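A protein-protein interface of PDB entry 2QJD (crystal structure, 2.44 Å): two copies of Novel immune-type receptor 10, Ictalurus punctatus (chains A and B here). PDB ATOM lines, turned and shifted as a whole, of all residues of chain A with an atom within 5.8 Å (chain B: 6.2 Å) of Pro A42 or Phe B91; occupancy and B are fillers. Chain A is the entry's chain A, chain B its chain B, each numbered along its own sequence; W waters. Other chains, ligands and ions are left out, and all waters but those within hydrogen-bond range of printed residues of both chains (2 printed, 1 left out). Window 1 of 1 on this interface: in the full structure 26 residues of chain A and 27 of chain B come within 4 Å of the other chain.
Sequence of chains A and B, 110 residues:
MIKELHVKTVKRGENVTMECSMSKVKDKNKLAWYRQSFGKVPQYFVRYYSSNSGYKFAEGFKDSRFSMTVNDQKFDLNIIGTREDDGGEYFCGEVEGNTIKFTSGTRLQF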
ATOM      1  N   TYR A  34       3.422 -15.978   5.647  1.00  0.00           N
ATOM      2  CA  TYR A  34       3.497 -14.562   5.990  1.00  0.00           C
ATOM      3  C   TYR A  34       4.141 -14.410   7.339  1.00  0.00           C
ATOM      4  O   TYR A  34       3.864 -15.155   8.267  1.00  0.00           O
ATOM      5  CB  TYR A  34       2.092 -13.876   5.965  1.00  0.00           C
ATOM      6  CG  TYR A  34       1.493 -14.007   4.593  1.00  0.00           C
ATOM      7  CD1 TYR A  34       1.362 -12.903   3.769  1.00  0.00           C
ATOM      8  CD2 TYR A  34       1.153 -15.247   4.083  1.00  0.00           C
ATOM      9  CE1 TYR A  34       0.888 -13.013   2.486  1.00  0.00           C
ATOM     10  CE2 TYR A  34       0.642 -15.391   2.784  1.00  0.00           C
ATOM     11  CZ  TYR A  34       0.501 -14.238   2.000  1.00  0.00           C
ATOM     12  OH  TYR A  34       0.030 -14.308   0.703  1.00  0.00           O
ATOM     13  N   ARG A  35       4.972 -13.396   7.426  1.00  0.00           N
ATOM     14  CA  ARG A  35       5.477 -12.951   8.675  1.00  0.00           C
ATOM     15  C   ARG A  35       4.871 -11.608   9.098  1.00  0.00           C
ATOM     16  O   ARG A  35       4.871 -10.650   8.327  1.00  0.00           O
ATOM     17  CB  ARG A  35       6.993 -12.825   8.587  1.00  0.00           C
ATOM     18  CG  ARG A  35       7.690 -12.561   9.903  1.00  0.00           C
ATOM     19  CD  ARG A  35       9.115 -12.360   9.515  1.00  0.00           C
ATOM     20  NE  ARG A  35       9.948 -12.104  10.678  1.00  0.00           N
ATOM     21  CZ  ARG A  35      11.286 -12.174  10.649  1.00  0.00           C
ATOM     22  NH1 ARG A  35      11.904 -12.507   9.500  1.00  0.00           N
ATOM     23  NH2 ARG A  35      11.996 -11.907  11.750  1.00  0.00           N
ATOM     24  N   GLN A  36       4.416 -11.544  10.356  1.00  0.00           N
ATOM     25  CA  GLN A  36       4.122 -10.243  10.973  1.00  0.00           C
ATOM     26  C   GLN A  36       5.010  -9.958  12.212  1.00  0.00           C
ATOM     27  O   GLN A  36       4.881 -10.653  13.200  1.00  0.00           O
ATOM     28  CB  GLN A  36       2.634 -10.147  11.325  1.00  0.00           C
ATOM     29  CG  GLN A  36       2.255  -8.828  11.741  1.00  0.00           C
ATOM     30  CD  GLN A  36       0.929  -8.772  12.431  1.00  0.00           C
ATOM     31  OE1 GLN A  36       0.336  -9.809  12.756  1.00  0.00           O
ATOM     32  NE2 GLN A  36       0.448  -7.540  12.714  1.00  0.00           N
ATOM     33  N   LYS A  40       3.889  -4.052  12.772  1.00  0.00           N
ATOM     34  CA  LYS A  40       3.927  -4.012  11.325  1.00  0.00           C
ATOM     35  C   LYS A  40       2.797  -4.834  10.724  1.00  0.00           C
ATOM     36  O   LYS A  40       2.146  -5.683  11.392  1.00  0.00           O
ATOM     37  CB  LYS A  40       5.275  -4.596  10.795  1.00  0.00           C
ATOM     38  CG  LYS A  40       6.584  -4.027  11.404  1.00  0.00           C
ATOM     39  CD  LYS A  40       7.079  -2.984  10.567  1.00  0.00           C
ATOM     40  CE  LYS A  40       7.952  -2.036  11.404  1.00  0.00           C
ATOM     41  NZ  LYS A  40       8.407  -0.920  10.506  1.00  0.00           N
ATOM     42  N   VAL A  41       2.576  -4.605   9.441  1.00  0.00           N
ATOM     43  CA  VAL A  41       1.550  -5.309   8.655  1.00  0.00           C
ATOM     44  C   VAL A  41       2.149  -6.695   8.311  1.00  0.00           C
ATOM     45  O   VAL A  41       3.363  -6.834   8.280  1.00  0.00           O
ATOM     46  CB  VAL A  41       1.248  -4.405   7.419  1.00  0.00           C
ATOM     47  CG1 VAL A  41       1.537  -5.057   6.079  1.00  0.00           C
ATOM     48  CG2 VAL A  41      -0.038  -3.635   7.579  1.00  0.00           C
ATOM     49  N   PRO A  42       1.308  -7.756   8.161  1.00  0.00           N
ATOM     50  CA  PRO A  42       1.973  -8.983   7.729  1.00  0.00           C
ATOM     51  C   PRO A  42       2.557  -8.853   6.330  1.00  0.00           C
ATOM     52  O   PRO A  42       2.127  -7.988   5.501  1.00  0.00           O
ATOM     53  CB  PRO A  42       0.862 -10.028   7.791  1.00  0.00           C
ATOM     54  CG  PRO A  42      -0.134  -9.422   8.833  1.00  0.00           C
ATOM     55  CD  PRO A  42      -0.115  -7.978   8.468  1.00  0.00           C
ATOM     56  N   GLN A  43       3.536  -9.713   6.064  1.00  0.00           N
ATOM     57  CA  GLN A  43       4.182  -9.682   4.782  1.00  0.00           C
ATOM     58  C   GLN A  43       4.550 -11.056   4.272  1.00  0.00           C
ATOM     59  O   GLN A  43       5.077 -11.894   5.026  1.00  0.00           O
ATOM     60  CB  GLN A  43       5.381  -8.725   4.804  1.00  0.00           C
ATOM     61  CG  GLN A  43       5.986  -8.698   3.431  1.00  0.00           C
ATOM     62  CD  GLN A  43       6.377  -7.333   2.942  1.00  0.00           C
ATOM     63  OE1 GLN A  43       5.575  -6.367   2.904  1.00  0.00           O
ATOM     64  NE2 GLN A  43       7.612  -7.250   2.498  1.00  0.00           N
ATOM     65  N   TYR A  44       4.292 -11.280   2.985  1.00  0.00           N
ATOM     66  CA  TYR A  44       4.566 -12.568   2.398  1.00  0.00           C
ATOM     67  C   TYR A  44       6.091 -12.738   2.314  1.00  0.00           C
ATOM     68  O   TYR A  44       6.786 -11.787   1.948  1.00  0.00           O
ATOM     69  CB  TYR A  44       3.882 -12.637   1.045  1.00  0.00           C
ATOM     70  CG  TYR A  44       4.778 -13.089  -0.073  1.00  0.00           C
ATOM     71  CD1 TYR A  44       5.114 -14.447  -0.201  1.00  0.00           C
ATOM     72  CD2 TYR A  44       5.322 -12.155  -0.987  1.00  0.00           C
ATOM     73  CE1 TYR A  44       5.958 -14.874  -1.208  1.00  0.00           C
ATOM     74  CE2 TYR A  44       6.177 -12.556  -2.006  1.00  0.00           C
ATOM     75  CZ  TYR A  44       6.482 -13.923  -2.110  1.00  0.00           C
ATOM     76  OH  TYR A  44       7.314 -14.393  -3.106  1.00  0.00           O
ATOM     77  N   PHE A  91       2.024 -16.815   9.444  1.00  0.00           N
ATOM     78  CA  PHE A  91       0.746 -17.431   9.019  1.00  0.00           C
ATOM     79  C   PHE A  91       0.904 -18.098   7.669  1.00  0.00           C
ATOM     80  O   PHE A  91       1.611 -17.599   6.736  1.00  0.00           O
ATOM     81  CB  PHE A  91      -0.427 -16.411   8.899  1.00  0.00           C
ATOM     82  CG  PHE A  91      -0.440 -15.367   9.964  1.00  0.00           C
ATOM     83  CD1 PHE A  91      -0.693 -15.708  11.301  1.00  0.00           C
ATOM     84  CD2 PHE A  91      -0.195 -14.040   9.636  1.00  0.00           C
ATOM     85  CE1 PHE A  91      -0.682 -14.728  12.283  1.00  0.00           C
ATOM     86  CE2 PHE A  91      -0.208 -13.052  10.624  1.00  0.00           C
ATOM     87  CZ  PHE A  91      -0.465 -13.387  11.917  1.00  0.00           C
ATOM     88  N   LYS B   3       5.218  -1.794   5.780  1.00  0.00           N
ATOM     89  CA  LYS B   3       4.223  -0.904   6.421  1.00  0.00           C
ATOM     90  C   LYS B   3       3.920  -0.986   7.966  1.00  0.00           C
ATOM     91  O   LYS B   3       3.519  -2.028   8.503  1.00  0.00           O
ATOM     92  CB  LYS B   3       2.927  -0.947   5.643  1.00  0.00           C
ATOM     93  CG  LYS B   3       2.057   0.232   5.958  1.00  0.00           C
ATOM     94  CD  LYS B   3       1.977   1.211   4.858  1.00  0.00           C
ATOM     95  CE  LYS B   3       0.625   2.031   4.941  1.00  0.00           C
ATOM     96  NZ  LYS B   3       0.441   2.666   6.274  1.00  0.00           N
ATOM     97  N   LEU B   5       1.805  -0.364  11.463  1.00  0.00           N
ATOM     98  CA  LEU B   5       0.401  -0.428  11.840  1.00  0.00           C
ATOM     99  C   LEU B   5      -0.016   0.901  12.524  1.00  0.00           C
ATOM    100  O   LEU B   5       0.763   1.495  13.252  1.00  0.00           O
ATOM    101  CB  LEU B   5       0.195  -1.578  12.815  1.00  0.00           C
ATOM    102  CG  LEU B   5       0.040  -3.030  12.338  1.00  0.00           C
ATOM    103  CD1 LEU B   5      -0.291  -3.755  13.602  1.00  0.00           C
ATOM    104  CD2 LEU B   5      -1.063  -3.298  11.284  1.00  0.00           C
ATOM    105  N   ALA B  32     -10.072  -6.683   0.806  1.00  0.00           N
ATOM    106  CA  ALA B  32     -10.883  -7.078   1.939  1.00  0.00           C
ATOM    107  C   ALA B  32     -10.254  -6.609   3.210  1.00  0.00           C
ATOM    108  O   ALA B  32      -9.081  -6.250   3.242  1.00  0.00           O
ATOM    109  CB  ALA B  32     -11.185  -8.571   1.946  1.00  0.00           C
ATOM    110  N   TRP B  33     -11.048  -6.538   4.276  1.00  0.00           N
ATOM    111  CA  TRP B  33     -10.482  -6.266   5.620  1.00  0.00           C
ATOM    112  C   TRP B  33     -10.284  -7.547   6.413  1.00  0.00           C
ATOM    113  O   TRP B  33     -11.174  -8.426   6.387  1.00  0.00           O
ATOM    114  CB  TRP B  33     -11.365  -5.266   6.381  1.00  0.00           C
ATOM    115  CG  TRP B  33     -10.985  -3.850   6.184  1.00  0.00           C
ATOM    116  CD1 TRP B  33     -11.590  -2.915   5.322  1.00  0.00           C
ATOM    117  CD2 TRP B  33      -9.921  -3.146   6.855  1.00  0.00           C
ATOM    118  NE1 TRP B  33     -10.960  -1.680   5.462  1.00  0.00           N
ATOM    119  CE2 TRP B  33      -9.940  -1.793   6.379  1.00  0.00           C
ATOM    120  CE3 TRP B  33      -9.003  -3.498   7.872  1.00  0.00           C
ATOM    121  CZ2 TRP B  33      -9.039  -0.821   6.850  1.00  0.00           C
ATOM    122  CZ3 TRP B  33      -8.091  -2.524   8.331  1.00  0.00           C
ATOM    123  CH2 TRP B  33      -8.119  -1.211   7.824  1.00  0.00           C
ATOM    124  N   TYR B  34      -9.145  -7.657   7.119  1.00  0.00           N
ATOM    125  CA  TYR B  34      -8.803  -8.907   7.911  1.00  0.00           C
ATOM    126  C   TYR B  34      -8.756  -8.672   9.402  1.00  0.00           C
ATOM    127  O   TYR B  34      -8.236  -7.651   9.830  1.00  0.00           O
ATOM    128  CB  TYR B  34      -7.503  -9.539   7.434  1.00  0.00           C
ATOM    129  CG  TYR B  34      -7.611 -10.041   6.018  1.00  0.00           C
ATOM    130  CD1 TYR B  34      -7.788 -11.406   5.754  1.00  0.00           C
ATOM    131  CD2 TYR B  34      -7.617  -9.146   4.953  1.00  0.00           C
ATOM    132  CE1 TYR B  34      -7.935 -11.854   4.483  1.00  0.00           C
ATOM    133  CE2 TYR B  34      -7.801  -9.578   3.632  1.00  0.00           C
ATOM    134  CZ  TYR B  34      -7.948 -10.928   3.411  1.00  0.00           C
ATOM    135  OH  TYR B  34      -8.110 -11.397   2.119  1.00  0.00           O
ATOM    136  N   ARG B  35      -9.346  -9.564  10.209  1.00  0.00           N
ATOM    137  CA  ARG B  35      -9.299  -9.391  11.635  1.00  0.00           C
ATOM    138  C   ARG B  35      -8.319 -10.408  12.204  1.00  0.00           C
ATOM    139  O   ARG B  35      -8.403 -11.593  11.834  1.00  0.00           O
ATOM    140  CB  ARG B  35     -10.660  -9.645  12.255  1.00  0.00           C
ATOM    141  CG  ARG B  35     -10.654  -9.567  13.862  1.00  0.00           C
ATOM    142  CD  ARG B  35     -11.908  -8.904  14.355  1.00  0.00           C
ATOM    143  NE  ARG B  35     -12.078  -8.998  15.799  1.00  0.00           N
ATOM    144  CZ  ARG B  35     -13.237  -8.782  16.464  1.00  0.00           C
ATOM    145  NH1 ARG B  35     -14.375  -8.416  15.822  1.00  0.00           N
ATOM    146  NH2 ARG B  35     -13.242  -8.938  17.796  1.00  0.00           N
ATOM    147  N   GLN B  36      -7.381  -9.959  13.061  1.00  0.00           N
ATOM    148  CA  GLN B  36      -6.539 -10.912  13.768  1.00  0.00           C
ATOM    149  C   GLN B  36      -6.623 -10.640  15.297  1.00  0.00           C
ATOM    150  O   GLN B  36      -5.999  -9.711  15.795  1.00  0.00           O
ATOM    151  CB  GLN B  36      -5.109 -10.867  13.237  1.00  0.00           C
ATOM    152  CG  GLN B  36      -4.285 -12.066  13.706  1.00  0.00           C
ATOM    153  CD  GLN B  36      -2.908 -11.839  14.313  1.00  0.00           C
ATOM    154  OE1 GLN B  36      -2.165 -10.800  14.182  1.00  0.00           O
ATOM    155  NE2 GLN B  36      -2.551 -12.840  15.024  1.00  0.00           N
ATOM    156  N   PRO B  42      -5.188 -14.578  11.060  1.00  0.00           N
ATOM    157  CA  PRO B  42      -6.120 -13.553  10.555  1.00  0.00           C
ATOM    158  C   PRO B  42      -7.304 -14.146   9.750  1.00  0.00           C
ATOM    159  O   PRO B  42      -7.207 -15.261   9.172  1.00  0.00           O
ATOM    160  CB  PRO B  42      -5.241 -12.678   9.678  1.00  0.00           C
ATOM    161  CG  PRO B  42      -3.826 -13.121   9.987  1.00  0.00           C
ATOM    162  CD  PRO B  42      -3.870 -14.503  10.416  1.00  0.00           C
ATOM    163  N   GLU B  89      -5.864  -6.630  15.874  1.00  0.00           N
ATOM    164  CA  GLU B  89      -5.302  -6.035  14.693  1.00  0.00           C
ATOM    165  C   GLU B  89      -6.239  -6.194  13.532  1.00  0.00           C
ATOM    166  O   GLU B  89      -7.026  -7.151  13.500  1.00  0.00           O
ATOM    167  CB  GLU B  89      -3.957  -6.689  14.378  1.00  0.00           C
ATOM    168  CG  GLU B  89      -2.958  -6.330  15.470  1.00  0.00           C
ATOM    169  CD  GLU B  89      -1.718  -7.104  15.403  1.00  0.00           C
ATOM    170  OE1 GLU B  89      -1.720  -8.102  14.644  1.00  0.00           O
ATOM    171  OE2 GLU B  89      -0.717  -6.648  16.014  1.00  0.00           O
ATOM    172  N   TYR B  90      -6.179  -5.230  12.594  1.00  0.00           N
ATOM    173  CA  TYR B  90      -7.088  -5.270  11.429  1.00  0.00           C
ATOM    174  C   TYR B  90      -6.221  -4.916  10.275  1.00  0.00           C
ATOM    175  O   TYR B  90      -5.424  -4.020  10.393  1.00  0.00           O
ATOM    176  CB  TYR B  90      -8.249  -4.273  11.609  1.00  0.00           C
ATOM    177  CG  TYR B  90      -9.212  -4.583  12.803  1.00  0.00           C
ATOM    178  CD1 TYR B  90     -10.472  -5.159  12.608  1.00  0.00           C
ATOM    179  CD2 TYR B  90      -8.832  -4.246  14.128  1.00  0.00           C
ATOM    180  CE1 TYR B  90     -11.346  -5.397  13.706  1.00  0.00           C
ATOM    181  CE2 TYR B  90      -9.634  -4.509  15.205  1.00  0.00           C
ATOM    182  CZ  TYR B  90     -10.887  -5.058  14.998  1.00  0.00           C
ATOM    183  OH  TYR B  90     -11.614  -5.243  16.126  1.00  0.00           O
ATOM    184  N   PHE B  91      -6.301  -5.643   9.177  1.00  0.00           N
ATOM    185  CA  PHE B  91      -5.382  -5.351   8.051  1.00  0.00           C
ATOM    186  C   PHE B  91      -6.192  -5.208   6.788  1.00  0.00           C
ATOM    187  O   PHE B  91      -7.174  -5.889   6.612  1.00  0.00           O
ATOM    188  CB  PHE B  91      -4.403  -6.496   7.779  1.00  0.00           C
ATOM    189  CG  PHE B  91      -3.801  -7.060   8.966  1.00  0.00           C
ATOM    190  CD1 PHE B  91      -3.140  -6.233   9.886  1.00  0.00           C
ATOM    191  CD2 PHE B  91      -3.915  -8.421   9.209  1.00  0.00           C
ATOM    192  CE1 PHE B  91      -2.572  -6.748  10.998  1.00  0.00           C
ATOM    193  CE2 PHE B  91      -3.346  -8.963  10.361  1.00  0.00           C
ATOM    194  CZ  PHE B  91      -2.669  -8.159  11.235  1.00  0.00           C
ATOM    195  N   CYS B  92      -5.783  -4.321   5.926  1.00  0.00           N
ATOM    196  CA  CYS B  92      -6.446  -4.219   4.639  1.00  0.00           C
ATOM    197  C   CYS B  92      -5.569  -4.970   3.645  1.00  0.00           C
ATOM    198  O   CYS B  92      -4.405  -4.617   3.448  1.00  0.00           O
ATOM    199  CB  CYS B  92      -6.522  -2.732   4.238  1.00  0.00           C
ATOM    200  SG  CYS B  92      -7.648  -2.458   2.872  1.00  0.00           S
ATOM    201  N   GLY B  93      -6.108  -6.033   3.070  1.00  0.00           N
ATOM    202  CA  GLY B  93      -5.378  -6.751   2.119  1.00  0.00           C
ATOM    203  C   GLY B  93      -5.919  -6.753   0.698  1.00  0.00           C
ATOM    204  O   GLY B  93      -7.141  -7.000   0.450  1.00  0.00           O
ATOM    205  N   ILE B 100      -1.275 -12.139  -1.181  1.00  0.00           N
ATOM    206  CA  ILE B 100      -1.938 -10.909  -0.782  1.00  0.00           C
ATOM    207  C   ILE B 100      -0.894  -9.911  -0.286  1.00  0.00           C
ATOM    208  O   ILE B 100       0.131 -10.293   0.300  1.00  0.00           O
ATOM    209  CB  ILE B 100      -2.997 -11.168   0.366  1.00  0.00           C
ATOM    210  CG1 ILE B 100      -3.922  -9.938   0.596  1.00  0.00           C
ATOM    211  CG2 ILE B 100      -2.281 -11.600   1.744  1.00  0.00           C
ATOM    212  CD1 ILE B 100      -5.304 -10.319   1.037  1.00  0.00           C
ATOM    213  N   LYS B 101      -1.134  -8.628  -0.541  1.00  0.00           N
ATOM    214  CA  LYS B 101      -0.314  -7.533  -0.001  1.00  0.00           C
ATOM    215  C   LYS B 101      -1.207  -6.792   1.010  1.00  0.00           C
ATOM    216  O   LYS B 101      -2.407  -6.573   0.721  1.00  0.00           O
ATOM    217  CB  LYS B 101       0.124  -6.576  -1.117  1.00  0.00           C
ATOM    218  CG  LYS B 101       0.995  -5.424  -0.627  1.00  0.00           C
ATOM    219  CD  LYS B 101       1.344  -4.359  -1.665  1.00  0.00           C
ATOM    220  CE  LYS B 101       0.086  -3.572  -2.259  1.00  0.00           C
ATOM    221  NZ  LYS B 101       0.405  -2.428  -3.330  1.00  0.00           N
ATOM    222  N   PHE B 102      -0.656  -6.448   2.183  1.00  0.00           N
ATOM    223  CA  PHE B 102      -1.385  -5.645   3.152  1.00  0.00           C
ATOM    224  C   PHE B 102      -0.896  -4.209   3.097  1.00  0.00           C
ATOM    225  O   PHE B 102       0.265  -3.914   3.325  1.00  0.00           O
ATOM    226  CB  PHE B 102      -1.381  -6.236   4.590  1.00  0.00           C
ATOM    227  CG  PHE B 102      -2.026  -7.598   4.676  1.00  0.00           C
ATOM    228  CD1 PHE B 102      -3.405  -7.722   4.760  1.00  0.00           C
ATOM    229  CD2 PHE B 102      -1.262  -8.734   4.645  1.00  0.00           C
ATOM    230  CE1 PHE B 102      -4.032  -8.945   4.807  1.00  0.00           C
ATOM    231  CE2 PHE B 102      -1.830  -9.960   4.668  1.00  0.00           C
ATOM    232  CZ  PHE B 102      -3.241 -10.079   4.773  1.00  0.00           C
ATOM    233  N   SER B 104      -2.172  -1.549   4.732  1.00  0.00           N
ATOM    234  CA  SER B 104      -2.726  -0.753   5.799  1.00  0.00           C
ATOM    235  C   SER B 104      -3.146  -1.663   6.922  1.00  0.00           C
ATOM    236  O   SER B 104      -3.612  -2.762   6.681  1.00  0.00           O
ATOM    237  CB  SER B 104      -4.008  -0.074   5.285  1.00  0.00           C
ATOM    238  OG  SER B 104      -3.961   1.244   5.755  1.00  0.00           O
ATOM    239  N   GLY B 105      -3.013  -1.192   8.149  1.00  0.00           N
ATOM    240  CA  GLY B 105      -3.568  -1.946   9.233  1.00  0.00           C
ATOM    241  C   GLY B 105      -3.671  -1.121  10.477  1.00  0.00           C
ATOM    242  O   GLY B 105      -2.888  -0.147  10.649  1.00  0.00           O
ATOM    243  N   THR B 106      -4.612  -1.485  11.347  1.00  0.00           N
ATOM    244  CA  THR B 106      -4.714  -0.827  12.640  1.00  0.00           C
ATOM    245  C   THR B 106      -4.637  -1.800  13.810  1.00  0.00           C
ATOM    246  O   THR B 106      -5.199  -2.893  13.769  1.00  0.00           O
ATOM    247  CB  THR B 106      -6.005  -0.010  12.745  1.00  0.00           C
ATOM    248  OG1 THR B 106      -5.953   1.015  11.758  1.00  0.00           O
ATOM    249  CG2 THR B 106      -6.202   0.626  14.125  1.00  0.00           C
HETATM  250  O   HOH W   1       2.077  -7.270   2.925  1.00  0.00           O
HETATM  251  O   HOH W   2       2.349  -9.492   1.487  1.00  0.00           O
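Pro A42 touches two residues of chain B. Of the printed residues of chain B, Phe A91 touches Gln B36 (3.8 Å) and Pro B42 (3.5 Å). Of the printed residues of chain A, Pro B42 touches Phe A91 (3.5 Å). Of chain A, only Gln A36 (3.5 Å) and Pro A42 (3.6 Å) come within 4 Å of Phe B91. Gly B93 touches none of the printed residues of chain A. Of the printed residues of chain A, Ile B100 touches Tyr A34. Printed residues of chain A within 4 Å of Ser B104: Val A41.
Water W2 bridges O of Ile B100 (2.6 Å) and N of Tyr A44 (3.0 Å). Water W1 bridges O of Pro A42 (2.7 Å) and N of Phe B102 (2.9 Å).
Printed residues of chain B that touch a printed residue of chain A: Lys B3, Leu B5, Gln B36, Pro B42, Glu B89, Phe B91, Ile B100, Phe B102, Ser B104 and Gly B105. Hydrophobic or aromatic side chains of chain B that line the printed part of chain A: Leu B5, Pro B42, Phe B91, Ile B100 and Phe B102. Hydrophobic or aromatic side chains of chain A that line the printed part of chain B: Tyr A34, Val A41, Pro A42 and Phe A91. Among the printed residues, no Asp or Glu carboxylate lies within 4 Å of a Lys or Arg side-chain nitrogen of the other chain.
The side-chain amide oxygen of Gln B36 sits close to the side-chain amide oxygen of Gln A36, at 3.0 Å. The side-chain hydroxyl (OH) of Tyr A34 is in hydrogen-bond range of the backbone NH (N) of Ile B100 (3.2 Å). OE1 of Glu B89 is in hydrogen-bond range of NE2 of Gln A36, at 3.0 Å. The backbone carbonyl oxygen of Lys B3 sits at hydrogen-bond distance from the backbone NH of Val A41 (2.9 Å).
Gln B36 touches its own counterpart, Gln A36. Gln A36 touches Phe B91, and with the chains exchanged Phe A91 touches Gln B36. Pro A42 touches Phe B91, and with the chains exchanged Phe A91 touches Pro B42. 5 positions are printed for both chains. Of the 16 pairs that touch across the chains among the printed residues, 5 have their exchanged pair printed and touching as well.
O of Ser B104 is in hydrogen-bond range of N of Cys B92 (2.8 Å). O of Phe A91 lies within hydrogen-bond range of N of Tyr A34 (2.7 Å). The side-chain carboxylate of Glu B89 lies close to the side-chain amide oxygen of Gln B36 (2.8 Å). The backbone carbonyl oxygen of Phe B91 sits at hydrogen-bond distance from the backbone NH of Tyr B34 (2.7 Å). The side-chain amide nitrogen (NE2) of Gln A36 is in hydrogen-bond range of the backbone carbonyl oxygen (O) of Lys A40 (2.8 Å).
Among the printed residues, pairs that only touch across the chains: Gln A36 with Leu B5 (3.96 Å), Gln A36 with Phe B91 (3.5 Å), Lys A40 with Lys B3 (3.5 Å), Lys A40 with Leu B5 (3.5 Å), Val A41 with Leu B5 (3.9 Å), Val A41 with Phe B102 (3.2 Å), Val A41 with Ser B104 (3.7 Å), Val A41 with Gly B105 (3.9 Å), Pro A42 with Phe B91 (3.6 Å), Pro A42 with Phe B102 (3.6 Å), Phe A91 with Gln B36 (3.8 Å) and Phe A91 with Pro B42 (3.5 Å).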
